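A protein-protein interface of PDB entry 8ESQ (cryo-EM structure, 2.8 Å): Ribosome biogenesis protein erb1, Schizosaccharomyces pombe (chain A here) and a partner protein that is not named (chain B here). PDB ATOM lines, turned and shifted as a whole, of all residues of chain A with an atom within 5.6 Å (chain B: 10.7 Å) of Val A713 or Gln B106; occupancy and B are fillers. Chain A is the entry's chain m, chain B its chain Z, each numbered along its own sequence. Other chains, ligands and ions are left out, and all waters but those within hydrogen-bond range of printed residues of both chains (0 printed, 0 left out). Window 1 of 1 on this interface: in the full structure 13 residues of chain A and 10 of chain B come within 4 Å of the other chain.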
ATOM      1  N   ARG A 385     -10.526   0.264  19.914  1.00  0.00           N
ATOM      2  CA  ARG A 385      -9.167   0.310  20.438  1.00  0.00           C
ATOM      3  C   ARG A 385      -8.832   1.711  20.932  1.00  0.00           C
ATOM      4  O   ARG A 385      -9.074   2.705  20.242  1.00  0.00           O
ATOM      5  CB  ARG A 385      -8.166  -0.112  19.362  1.00  0.00           C
ATOM      6  CG  ARG A 385      -8.497  -1.419  18.667  1.00  0.00           C
ATOM      7  CD  ARG A 385      -7.523  -1.699  17.537  1.00  0.00           C
ATOM      8  NE  ARG A 385      -7.346  -0.538  16.674  1.00  0.00           N
ATOM      9  CZ  ARG A 385      -6.628  -0.535  15.559  1.00  0.00           C
ATOM     10  NH1 ARG A 385      -6.003  -1.622  15.138  1.00  0.00           N
ATOM     11  NH2 ARG A 385      -6.534   0.586  14.850  1.00  0.00           N
ATOM     12  N   ARG A 661       5.067  -2.148  21.593  1.00  0.00           N
ATOM     13  CA  ARG A 661       4.309  -0.988  21.133  1.00  0.00           C
ATOM     14  C   ARG A 661       4.811   0.305  21.764  1.00  0.00           C
ATOM     15  O   ARG A 661       5.238   1.226  21.059  1.00  0.00           O
ATOM     16  CB  ARG A 661       2.822  -1.186  21.431  1.00  0.00           C
ATOM     17  CG  ARG A 661       2.227  -2.423  20.788  1.00  0.00           C
ATOM     18  CD  ARG A 661       2.735  -2.617  19.373  1.00  0.00           C
ATOM     19  NE  ARG A 661       2.420  -1.469  18.533  1.00  0.00           N
ATOM     20  CZ  ARG A 661       1.310  -1.363  17.819  1.00  0.00           C
ATOM     21  NH1 ARG A 661       0.377  -2.298  17.856  1.00  0.00           N
ATOM     22  NH2 ARG A 661       1.126  -0.286  17.060  1.00  0.00           N
ATOM     23  N   ASP A 677       1.958  -5.930  21.576  1.00  0.00           N
ATOM     24  CA  ASP A 677       0.749  -6.511  21.005  1.00  0.00           C
ATOM     25  C   ASP A 677       0.396  -7.857  21.622  1.00  0.00           C
ATOM     26  O   ASP A 677      -0.721  -8.341  21.419  1.00  0.00           O
ATOM     27  CB  ASP A 677       0.900  -6.663  19.492  1.00  0.00           C
ATOM     28  CG  ASP A 677       0.794  -5.342  18.760  1.00  0.00           C
ATOM     29  OD1 ASP A 677       0.054  -4.457  19.236  1.00  0.00           O
ATOM     30  OD2 ASP A 677       1.452  -5.186  17.710  1.00  0.00           O
ATOM     31  N   LYS A 708      -6.836  -8.344  26.851  1.00  0.00           N
ATOM     32  CA  LYS A 708      -7.388  -8.876  25.614  1.00  0.00           C
ATOM     33  C   LYS A 708      -6.510  -8.519  24.416  1.00  0.00           C
ATOM     34  O   LYS A 708      -5.745  -7.551  24.432  1.00  0.00           O
ATOM     35  CB  LYS A 708      -8.805  -8.347  25.392  1.00  0.00           C
ATOM     36  CG  LYS A 708      -9.744  -8.578  26.562  1.00  0.00           C
ATOM     37  CD  LYS A 708     -11.046  -7.817  26.379  1.00  0.00           C
ATOM     38  CE  LYS A 708     -11.910  -7.897  27.625  1.00  0.00           C
ATOM     39  NZ  LYS A 708     -13.100  -7.008  27.533  1.00  0.00           N
ATOM     40  N   VAL A 709      -6.632  -9.328  23.365  1.00  0.00           N
ATOM     41  CA  VAL A 709      -5.956  -9.099  22.094  1.00  0.00           C
ATOM     42  C   VAL A 709      -7.007  -9.085  20.993  1.00  0.00           C
ATOM     43  O   VAL A 709      -7.785 -10.037  20.859  1.00  0.00           O
ATOM     44  CB  VAL A 709      -4.887 -10.171  21.812  1.00  0.00           C
ATOM     45  CG1 VAL A 709      -4.199  -9.897  20.485  1.00  0.00           C
ATOM     46  CG2 VAL A 709      -3.872 -10.218  22.943  1.00  0.00           C
ATOM     47  N   VAL A 710      -7.029  -8.010  20.207  1.00  0.00           N
ATOM     48  CA  VAL A 710      -8.010  -7.822  19.145  1.00  0.00           C
ATOM     49  C   VAL A 710      -7.270  -7.476  17.861  1.00  0.00           C
ATOM     50  O   VAL A 710      -6.451  -6.552  17.847  1.00  0.00           O
ATOM     51  CB  VAL A 710      -9.024  -6.716  19.494  1.00  0.00           C
ATOM     52  CG1 VAL A 710      -9.943  -6.441  18.312  1.00  0.00           C
ATOM     53  CG2 VAL A 710      -9.825  -7.095  20.729  1.00  0.00           C
ATOM     54  N   ASP A 711      -7.573  -8.205  16.784  1.00  0.00           N
ATOM     55  CA  ASP A 711      -6.958  -7.973  15.475  1.00  0.00           C
ATOM     56  C   ASP A 711      -5.434  -8.018  15.559  1.00  0.00           C
ATOM     57  O   ASP A 711      -4.734  -7.203  14.956  1.00  0.00           O
ATOM     58  CB  ASP A 711      -7.425  -6.643  14.876  1.00  0.00           C
ATOM     59  CG  ASP A 711      -8.908  -6.627  14.573  1.00  0.00           C
ATOM     60  OD1 ASP A 711      -9.489  -7.715  14.374  1.00  0.00           O
ATOM     61  OD2 ASP A 711      -9.494  -5.525  14.531  1.00  0.00           O
ATOM     62  N   ASN A 712      -4.918  -8.985  16.322  1.00  0.00           N
ATOM     63  CA  ASN A 712      -3.483  -9.114  16.582  1.00  0.00           C
ATOM     64  C   ASN A 712      -2.910  -7.852  17.222  1.00  0.00           C
ATOM     65  O   ASN A 712      -1.754  -7.494  16.984  1.00  0.00           O
ATOM     66  CB  ASN A 712      -2.708  -9.460  15.307  1.00  0.00           C
ATOM     67  CG  ASN A 712      -3.242 -10.698  14.619  1.00  0.00           C
ATOM     68  OD1 ASN A 712      -2.797 -11.812  14.890  1.00  0.00           O
ATOM     69  ND2 ASN A 712      -4.204 -10.509  13.723  1.00  0.00           N
ATOM     70  N   VAL A 713      -3.712  -7.165  18.033  1.00  0.00           N
ATOM     71  CA  VAL A 713      -3.286  -5.956  18.728  1.00  0.00           C
ATOM     72  C   VAL A 713      -3.555  -6.146  20.211  1.00  0.00           C
ATOM     73  O   VAL A 713      -4.659  -6.546  20.598  1.00  0.00           O
ATOM     74  CB  VAL A 713      -4.014  -4.701  18.212  1.00  0.00           C
ATOM     75  CG1 VAL A 713      -3.474  -3.445  18.894  1.00  0.00           C
ATOM     76  CG2 VAL A 713      -3.925  -4.610  16.701  1.00  0.00           C
ATOM     77  N   GLY A 714      -2.554  -5.857  21.035  1.00  0.00           N
ATOM     78  CA  GLY A 714      -2.708  -5.942  22.473  1.00  0.00           C
ATOM     79  C   GLY A 714      -2.642  -4.588  23.146  1.00  0.00           C
ATOM     80  O   GLY A 714      -3.442  -3.698  22.846  1.00  0.00           O
ATOM     81  N   VAL A 715      -1.691  -4.421  24.065  1.00  0.00           N
ATOM     82  CA  VAL A 715      -1.535  -3.143  24.749  1.00  0.00           C
ATOM     83  C   VAL A 715      -0.981  -2.124  23.767  1.00  0.00           C
ATOM     84  O   VAL A 715       0.090  -2.324  23.180  1.00  0.00           O
ATOM     85  CB  VAL A 715      -0.629  -3.293  25.972  1.00  0.00           C
ATOM     86  CG1 VAL A 715      -0.700  -2.045  26.838  1.00  0.00           C
ATOM     87  CG2 VAL A 715      -1.017  -4.530  26.763  1.00  0.00           C
ATOM     88  N   LEU A 716      -1.706  -1.023  23.582  1.00  0.00           N
ATOM     89  CA  LEU A 716      -1.291   0.005  22.636  1.00  0.00           C
ATOM     90  C   LEU A 716      -0.466   1.101  23.302  1.00  0.00           C
ATOM     91  O   LEU A 716       0.591   1.481  22.792  1.00  0.00           O
ATOM     92  CB  LEU A 716      -2.516   0.613  21.948  1.00  0.00           C
ATOM     93  CG  LEU A 716      -2.959  -0.067  20.653  1.00  0.00           C
ATOM     94  CD1 LEU A 716      -4.108   0.696  20.016  1.00  0.00           C
ATOM     95  CD2 LEU A 716      -1.792  -0.191  19.689  1.00  0.00           C
ATOM     96  N   ALA A 732      -6.744  -3.095  23.119  1.00  0.00           N
ATOM     97  CA  ALA A 732      -7.439  -3.043  21.841  1.00  0.00           C
ATOM     98  C   ALA A 732      -8.922  -3.363  21.963  1.00  0.00           C
ATOM     99  O   ALA A 732      -9.662  -3.163  20.995  1.00  0.00           O
ATOM    100  CB  ALA A 732      -6.785  -4.003  20.846  1.00  0.00           C
ATOM    101  N   VAL B  42      -1.366  -2.646  -3.631  1.00  0.00           N
ATOM    102  CA  VAL B  42      -0.782  -3.619  -2.719  1.00  0.00           C
ATOM    103  C   VAL B  42      -0.630  -4.950  -3.439  1.00  0.00           C
ATOM    104  O   VAL B  42      -1.571  -5.442  -4.074  1.00  0.00           O
ATOM    105  CB  VAL B  42      -1.646  -3.774  -1.462  1.00  0.00           C
ATOM    106  CG1 VAL B  42      -1.089  -4.885  -0.603  1.00  0.00           C
ATOM    107  CG2 VAL B  42      -1.716  -2.466  -0.696  1.00  0.00           C
ATOM    108  N   ILE B  72       4.553  -8.841   1.173  1.00  0.00           N
ATOM    109  CA  ILE B  72       3.473  -7.910   0.873  1.00  0.00           C
ATOM    110  C   ILE B  72       4.077  -6.520   0.746  1.00  0.00           C
ATOM    111  O   ILE B  72       4.833  -6.082   1.621  1.00  0.00           O
ATOM    112  CB  ILE B  72       2.376  -7.949   1.951  1.00  0.00           C
ATOM    113  CG1 ILE B  72       2.995  -7.896   3.349  1.00  0.00           C
ATOM    114  CG2 ILE B  72       1.521  -9.196   1.794  1.00  0.00           C
ATOM    115  CD1 ILE B  72       1.982  -7.737   4.459  1.00  0.00           C
ATOM    116  N   GLY B  94      -9.753  -9.096   0.991  1.00  0.00           N
ATOM    117  CA  GLY B  94     -10.033  -8.172   2.066  1.00  0.00           C
ATOM    118  C   GLY B  94      -9.126  -8.278   3.270  1.00  0.00           C
ATOM    119  O   GLY B  94      -9.264  -7.472   4.200  1.00  0.00           O
ATOM    120  N   LEU B  95      -8.201  -9.242   3.291  1.00  0.00           N
ATOM    121  CA  LEU B  95      -7.268  -9.335   4.409  1.00  0.00           C
ATOM    122  C   LEU B  95      -6.364  -8.110   4.472  1.00  0.00           C
ATOM    123  O   LEU B  95      -5.892  -7.731   5.549  1.00  0.00           O
ATOM    124  CB  LEU B  95      -6.442 -10.621   4.304  1.00  0.00           C
ATOM    125  CG  LEU B  95      -5.080 -10.597   3.604  1.00  0.00           C
ATOM    126  CD1 LEU B  95      -4.415 -11.944   3.744  1.00  0.00           C
ATOM    127  CD2 LEU B  95      -5.224 -10.260   2.130  1.00  0.00           C
ATOM    128  N   ILE B  96      -6.116  -7.482   3.332  1.00  0.00           N
ATOM    129  CA  ILE B  96      -5.194  -6.359   3.254  1.00  0.00           C
ATOM    130  C   ILE B  96      -5.954  -5.051   3.445  1.00  0.00           C
ATOM    131  O   ILE B  96      -7.113  -4.915   3.036  1.00  0.00           O
ATOM    132  CB  ILE B  96      -4.443  -6.393   1.907  1.00  0.00           C
ATOM    133  CG1 ILE B  96      -3.149  -5.589   1.986  1.00  0.00           C
ATOM    134  CG2 ILE B  96      -5.325  -5.893   0.766  1.00  0.00           C
ATOM    135  CD1 ILE B  96      -2.348  -5.832   3.228  1.00  0.00           C
ATOM    136  N   THR B  97      -5.300  -4.083   4.086  1.00  0.00           N
ATOM    137  CA  THR B  97      -5.859  -2.745   4.257  1.00  0.00           C
ATOM    138  C   THR B  97      -4.793  -1.833   4.845  1.00  0.00           C
ATOM    139  O   THR B  97      -3.661  -2.248   5.108  1.00  0.00           O
ATOM    140  CB  THR B  97      -7.099  -2.736   5.156  1.00  0.00           C
ATOM    141  OG1 THR B  97      -7.583  -1.393   5.285  1.00  0.00           O
ATOM    142  CG2 THR B  97      -6.761  -3.283   6.525  1.00  0.00           C
ATOM    143  N   ALA B  98      -5.185  -0.574   5.055  1.00  0.00           N
ATOM    144  CA  ALA B  98      -4.283   0.404   5.649  1.00  0.00           C
ATOM    145  C   ALA B  98      -3.863  -0.009   7.054  1.00  0.00           C
ATOM    146  O   ALA B  98      -2.706   0.187   7.443  1.00  0.00           O
ATOM    147  CB  ALA B  98      -4.946   1.780   5.670  1.00  0.00           C
ATOM    148  N   ASP B  99      -4.787  -0.577   7.832  1.00  0.00           N
ATOM    149  CA  ASP B  99      -4.456  -0.999   9.189  1.00  0.00           C
ATOM    150  C   ASP B  99      -3.374  -2.071   9.196  1.00  0.00           C
ATOM    151  O   ASP B  99      -2.463  -2.041  10.033  1.00  0.00           O
ATOM    152  CB  ASP B  99      -5.709  -1.508   9.903  1.00  0.00           C
ATOM    153  CG  ASP B  99      -5.553  -1.524  11.411  1.00  0.00           C
ATOM    154  OD1 ASP B  99      -4.661  -0.818  11.923  1.00  0.00           O
ATOM    155  OD2 ASP B  99      -6.322  -2.240  12.087  1.00  0.00           O
ATOM    156  N   THR B 100      -3.465  -3.036   8.283  1.00  0.00           N
ATOM    157  CA  THR B 100      -2.495  -4.124   8.252  1.00  0.00           C
ATOM    158  C   THR B 100      -1.092  -3.630   7.915  1.00  0.00           C
ATOM    159  O   THR B 100      -0.110  -4.082   8.514  1.00  0.00           O
ATOM    160  CB  THR B 100      -2.948  -5.185   7.256  1.00  0.00           C
ATOM    161  OG1 THR B 100      -2.915  -4.630   5.939  1.00  0.00           O
ATOM    162  CG2 THR B 100      -4.347  -5.665   7.578  1.00  0.00           C
ATOM    163  N   PHE B 101      -0.971  -2.712   6.958  1.00  0.00           N
ATOM    164  CA  PHE B 101       0.349  -2.185   6.637  1.00  0.00           C
ATOM    165  C   PHE B 101       0.850  -1.176   7.658  1.00  0.00           C
ATOM    166  O   PHE B 101       2.036  -0.832   7.630  1.00  0.00           O
ATOM    167  CB  PHE B 101       0.362  -1.545   5.247  1.00  0.00           C
ATOM    168  CG  PHE B 101       1.085  -2.362   4.212  1.00  0.00           C
ATOM    169  CD1 PHE B 101       0.786  -3.699   4.020  1.00  0.00           C
ATOM    170  CD2 PHE B 101       2.065  -1.781   3.424  1.00  0.00           C
ATOM    171  CE1 PHE B 101       1.460  -4.445   3.062  1.00  0.00           C
ATOM    172  CE2 PHE B 101       2.746  -2.522   2.473  1.00  0.00           C
ATOM    173  CZ  PHE B 101       2.440  -3.852   2.289  1.00  0.00           C
ATOM    174  N   LYS B 102      -0.012  -0.693   8.550  1.00  0.00           N
ATOM    175  CA  LYS B 102       0.430   0.162   9.643  1.00  0.00           C
ATOM    176  C   LYS B 102       0.814  -0.650  10.873  1.00  0.00           C
ATOM    177  O   LYS B 102       1.861  -0.405  11.481  1.00  0.00           O
ATOM    178  CB  LYS B 102      -0.658   1.183   9.993  1.00  0.00           C
ATOM    179  CG  LYS B 102      -0.914   2.240   8.920  1.00  0.00           C
ATOM    180  CD  LYS B 102       0.266   3.191   8.765  1.00  0.00           C
ATOM    181  CE  LYS B 102       1.094   2.875   7.526  1.00  0.00           C
ATOM    182  NZ  LYS B 102       2.190   3.862   7.324  1.00  0.00           N
ATOM    183  N   GLU B 103      -0.012  -1.615  11.248  1.00  0.00           N
ATOM    184  CA  GLU B 103       0.229  -2.379  12.464  1.00  0.00           C
ATOM    185  C   GLU B 103       1.246  -3.485  12.205  1.00  0.00           C
ATOM    186  O   GLU B 103       0.982  -4.375  11.384  1.00  0.00           O
ATOM    187  CB  GLU B 103      -1.085  -2.952  12.975  1.00  0.00           C
ATOM    188  CG  GLU B 103      -1.728  -2.059  14.013  1.00  0.00           C
ATOM    189  CD  GLU B 103      -1.320  -2.410  15.422  1.00  0.00           C
ATOM    190  OE1 GLU B 103      -0.201  -2.934  15.612  1.00  0.00           O
ATOM    191  OE2 GLU B 103      -2.095  -2.114  16.351  1.00  0.00           O
ATOM    192  N   PRO B 104       2.408  -3.468  12.865  1.00  0.00           N
ATOM    193  CA  PRO B 104       3.442  -4.474  12.558  1.00  0.00           C
ATOM    194  C   PRO B 104       2.999  -5.905  12.799  1.00  0.00           C
ATOM    195  O   PRO B 104       3.369  -6.799  12.027  1.00  0.00           O
ATOM    196  CB  PRO B 104       4.601  -4.075  13.484  1.00  0.00           C
ATOM    197  CG  PRO B 104       4.326  -2.659  13.863  1.00  0.00           C
ATOM    198  CD  PRO B 104       2.843  -2.528  13.908  1.00  0.00           C
ATOM    199  N   THR B 105       2.220  -6.154  13.852  1.00  0.00           N
ATOM    200  CA  THR B 105       1.745  -7.512  14.099  1.00  0.00           C
ATOM    201  C   THR B 105       0.748  -7.945  13.033  1.00  0.00           C
ATOM    202  O   THR B 105       0.757  -9.104  12.601  1.00  0.00           O
ATOM    203  CB  THR B 105       1.125  -7.611  15.491  1.00  0.00           C
ATOM    204  OG1 THR B 105       1.993  -6.987  16.443  1.00  0.00           O
ATOM    205  CG2 THR B 105       0.929  -9.068  15.879  1.00  0.00           C
ATOM    206  N   GLN B 106      -0.120  -7.029  12.601  1.00  0.00           N
ATOM    207  CA  GLN B 106      -1.025  -7.332  11.498  1.00  0.00           C
ATOM    208  C   GLN B 106      -0.251  -7.591  10.213  1.00  0.00           C
ATOM    209  O   GLN B 106      -0.607  -8.481   9.432  1.00  0.00           O
ATOM    210  CB  GLN B 106      -2.023  -6.191  11.313  1.00  0.00           C
ATOM    211  CG  GLN B 106      -3.190  -6.241  12.281  1.00  0.00           C
ATOM    212  CD  GLN B 106      -4.083  -5.023  12.181  1.00  0.00           C
ATOM    213  OE1 GLN B 106      -3.863  -4.147  11.347  1.00  0.00           O
ATOM    214  NE2 GLN B 106      -5.096  -4.960  13.037  1.00  0.00           N
ATOM    215  N   ARG B 107       0.811  -6.816   9.974  1.00  0.00           N
ATOM    216  CA  ARG B 107       1.680  -7.087   8.833  1.00  0.00           C
ATOM    217  C   ARG B 107       2.316  -8.465   8.947  1.00  0.00           C
ATOM    218  O   ARG B 107       2.369  -9.217   7.966  1.00  0.00           O
ATOM    219  CB  ARG B 107       2.759  -6.012   8.725  1.00  0.00           C
ATOM    220  CG  ARG B 107       3.725  -6.230   7.576  1.00  0.00           C
ATOM    221  CD  ARG B 107       4.743  -5.107   7.479  1.00  0.00           C
ATOM    222  NE  ARG B 107       4.154  -3.862   7.006  1.00  0.00           N
ATOM    223  CZ  ARG B 107       4.849  -2.772   6.711  1.00  0.00           C
ATOM    224  NH1 ARG B 107       6.167  -2.740   6.826  1.00  0.00           N
ATOM    225  NH2 ARG B 107       4.208  -1.687   6.287  1.00  0.00           N
ATOM    226  N   SER B 108       2.805  -8.815  10.139  1.00  0.00           N
ATOM    227  CA  SER B 108       3.360 -10.147  10.346  1.00  0.00           C
ATOM    228  C   SER B 108       2.290 -11.217  10.187  1.00  0.00           C
ATOM    229  O   SER B 108       2.548 -12.284   9.616  1.00  0.00           O
ATOM    230  CB  SER B 108       4.009 -10.238  11.726  1.00  0.00           C
ATOM    231  OG  SER B 108       3.145 -10.878  12.648  1.00  0.00           O
ATOM    232  N   ALA B 109       1.084 -10.956  10.698  1.00  0.00           N
ATOM    233  CA  ALA B 109      -0.010 -11.908  10.530  1.00  0.00           C
ATOM    234  C   ALA B 109      -0.381 -12.065   9.062  1.00  0.00           C
ATOM    235  O   ALA B 109      -0.622 -13.182   8.594  1.00  0.00           O
ATOM    236  CB  ALA B 109      -1.224 -11.467  11.346  1.00  0.00           C
ATOM    237  N   ALA B 110      -0.425 -10.956   8.320  1.00  0.00           N
ATOM    238  CA  ALA B 110      -0.747 -11.033   6.899  1.00  0.00           C
ATOM    239  C   ALA B 110       0.292 -11.853   6.148  1.00  0.00           C
ATOM    240  O   ALA B 110      -0.050 -12.629   5.249  1.00  0.00           O
ATOM    241  CB  ALA B 110      -0.858  -9.629   6.305  1.00  0.00           C
ATOM    242  N   ARG B 111       1.568 -11.696   6.505  1.00  0.00           N
ATOM    243  CA  ARG B 111       2.616 -12.493   5.878  1.00  0.00           C
ATOM    244  C   ARG B 111       2.453 -13.974   6.197  1.00  0.00           C
ATOM    245  O   ARG B 111       2.812 -14.832   5.382  1.00  0.00           O
ATOM    246  CB  ARG B 111       3.991 -11.990   6.314  1.00  0.00           C
ATOM    247  CG  ARG B 111       4.338 -10.619   5.760  1.00  0.00           C
ATOM    248  CD  ARG B 111       5.718 -10.167   6.199  1.00  0.00           C
ATOM    249  NE  ARG B 111       6.014  -8.821   5.722  1.00  0.00           N
ATOM    250  CZ  ARG B 111       7.089  -8.123   6.059  1.00  0.00           C
ATOM    251  NH1 ARG B 111       7.992  -8.606   6.895  1.00  0.00           N
ATOM    252  NH2 ARG B 111       7.261  -6.910   5.544  1.00  0.00           N
ATOM    253  N   LYS B 112       1.930 -14.297   7.382  1.00  0.00           N
ATOM    254  CA  LYS B 112       1.691 -15.697   7.719  1.00  0.00           C
ATOM    255  C   LYS B 112       0.623 -16.316   6.822  1.00  0.00           C
ATOM    256  O   LYS B 112       0.821 -17.410   6.282  1.00  0.00           O
ATOM    257  CB  LYS B 112       1.296 -15.832   9.189  1.00  0.00           C
ATOM    258  CG  LYS B 112       2.405 -15.519  10.181  1.00  0.00           C
ATOM    259  CD  LYS B 112       1.961 -15.840  11.601  1.00  0.00           C
ATOM    260  CE  LYS B 112       3.062 -15.569  12.612  1.00  0.00           C
ATOM    261  NZ  LYS B 112       3.341 -14.115  12.755  1.00  0.00           N
ATOM    262  N   THR B 113      -0.516 -15.637   6.654  1.00  0.00           N
ATOM    263  CA  THR B 113      -1.606 -16.215   5.871  1.00  0.00           C
ATOM    264  C   THR B 113      -1.234 -16.350   4.401  1.00  0.00           C
ATOM    265  O   THR B 113      -1.527 -17.376   3.773  1.00  0.00           O
ATOM    266  CB  THR B 113      -2.878 -15.382   6.013  1.00  0.00           C
ATOM    267  OG1 THR B 113      -2.886 -14.351   5.019  1.00  0.00           O
ATOM    268  CG2 THR B 113      -2.985 -14.770   7.396  1.00  0.00           C
ATOM    269  N   VAL B 114      -0.606 -15.323   3.824  1.00  0.00           N
ATOM    270  CA  VAL B 114      -0.228 -15.401   2.415  1.00  0.00           C
ATOM    271  C   VAL B 114       0.801 -16.502   2.207  1.00  0.00           C
ATOM    272  O   VAL B 114       0.856 -17.128   1.142  1.00  0.00           O
ATOM    273  CB  VAL B 114       0.282 -14.037   1.909  1.00  0.00           C
ATOM    274  CG1 VAL B 114      -0.809 -12.989   2.022  1.00  0.00           C
ATOM    275  CG2 VAL B 114       1.524 -13.608   2.661  1.00  0.00           C
ATOM    276  N   LYS B 115       1.637 -16.754   3.217  1.00  0.00           N
ATOM    277  CA  LYS B 115       2.515 -17.915   3.163  1.00  0.00           C
ATOM    278  C   LYS B 115       1.709 -19.206   3.207  1.00  0.00           C
ATOM    279  O   LYS B 115       1.910 -20.097   2.376  1.00  0.00           O
ATOM    280  CB  LYS B 115       3.525 -17.874   4.309  1.00  0.00           C
ATOM    281  CG  LYS B 115       4.406 -19.109   4.383  1.00  0.00           C
ATOM    282  CD  LYS B 115       5.336 -19.068   5.581  1.00  0.00           C
ATOM    283  CE  LYS B 115       6.561 -18.222   5.289  1.00  0.00           C
ATOM    284  NZ  LYS B 115       7.484 -18.893   4.336  1.00  0.00           N
ATOM    285  N   LYS B 116       0.774 -19.310   4.156  1.00  0.00           N
ATOM    286  CA  LYS B 116      -0.013 -20.532   4.292  1.00  0.00           C
ATOM    287  C   LYS B 116      -0.821 -20.814   3.033  1.00  0.00           C
ATOM    288  O   LYS B 116      -0.933 -21.969   2.605  1.00  0.00           O
ATOM    289  CB  LYS B 116      -0.937 -20.434   5.505  1.00  0.00           C
ATOM    290  CG  LYS B 116      -0.216 -20.414   6.841  1.00  0.00           C
ATOM    291  CD  LYS B 116      -1.196 -20.525   8.000  1.00  0.00           C
ATOM    292  CE  LYS B 116      -2.008 -19.251   8.174  1.00  0.00           C
ATOM    293  NZ  LYS B 116      -1.174 -18.116   8.656  1.00  0.00           N
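O of Asp B99 lies close to OE1 of Gln B106 (2.8 Å). N of Thr B100 is in hydrogen-bond range of OE1 of Gln B106, at 3.3 Å. OG of Ser B108 lies within hydrogen-bond range of O of Thr B105 (3.0 Å). The side-chain carboxylate (OD1) of Asp A677 lies within salt-bridge range of the guanidinium group (NH1) of Arg A661 (2.6 Å). O of Asp A677 lies within hydrogen-bond range of N of Gly A714 (3.1 Å).
OD2 of Asp B99 is in salt-bridge range of NH1 of Arg A385, 3.1 Å away. The side-chain carboxylate (OE1) of Glu B103 lies within salt-bridge range of the guanidinium group (NH1) of Arg A661. NE2 of Gln B106 sits at hydrogen-bond distance from O of Asp A711. OD2 of Asp A677 lies close to OE1 of Glu B103 (3.5 Å). The side-chain carboxylate of Asp A677 sits close to the side-chain hydroxyl of Thr B105.
Printed residues of chain B within 4 Å of Arg A661: Glu B103. Asp A677 touches just these residues of chain B: Glu B103 (3.5 Å) and Thr B105 (2.3 Å). No residue of chain B comes within 4 Å of Val A709. No residue of chain B comes within 4 Å of Val A710. Asp A711 touches just one residue of chain B: Gln B106. Val A713 touches just these residues of chain B: Glu B103 and Gln B106. No residue of chain B comes within 4 Å of Gly A714. No residue of chain B comes within 4 Å of Ala A732. Of the printed residues of chain A, Asp B99 touches Arg A385. Printed residues of chain A within 4 Å of Glu B103: Arg A661 (2.4 Å), Asp A677 (3.5 Å), Val A713 (3.1 Å) and Leu A716 (3.9 Å). Of the printed residues of chain A, Thr B105 touches Asp A677 (2.3 Å) and Asn A712 (3.2 Å). Of chain A, only Asp A711 and Val A713 come within 4 Å of Gln B106. Printed residues of chain A within 4 Å of Ala B109: Asn A712. The nearest residue of chain B that does not touch Val A713 is Thr B105 (5.5 Å). The nearest printed residue of chain A that does not touch Thr B105 is Arg A661 (5.2 Å).
Printed residues of chain B that touch a printed residue of chain A: Asp B99, Glu B103, Thr B105, Gln B106 and Ala B109. Hydrophobic or aromatic side chains of chain B that line the printed part of chain A: Ala B109. Of the 13 printed residues of chain A, 7 touch a printed residue of chain B. Among the printed residues, 10 pairs touch across the chains. Among the printed residues, Asp or Glu carboxylates within 4 Å of a Lys or Arg side-chain nitrogen of the other chain: Arg A385 with Asp B99 and Arg A661 with Glu B103.
Asn A712 touches Thr B105. Asn A712 touches Ala B109 (OD1 to CB, 3.9 Å). Val A713 touches Glu B103 (CG2 to OE2, 3.1 Å). Val A713 touches Gln B106. Leu A716 touches Glu B103 (CD2 to OE2, 3.9 Å).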
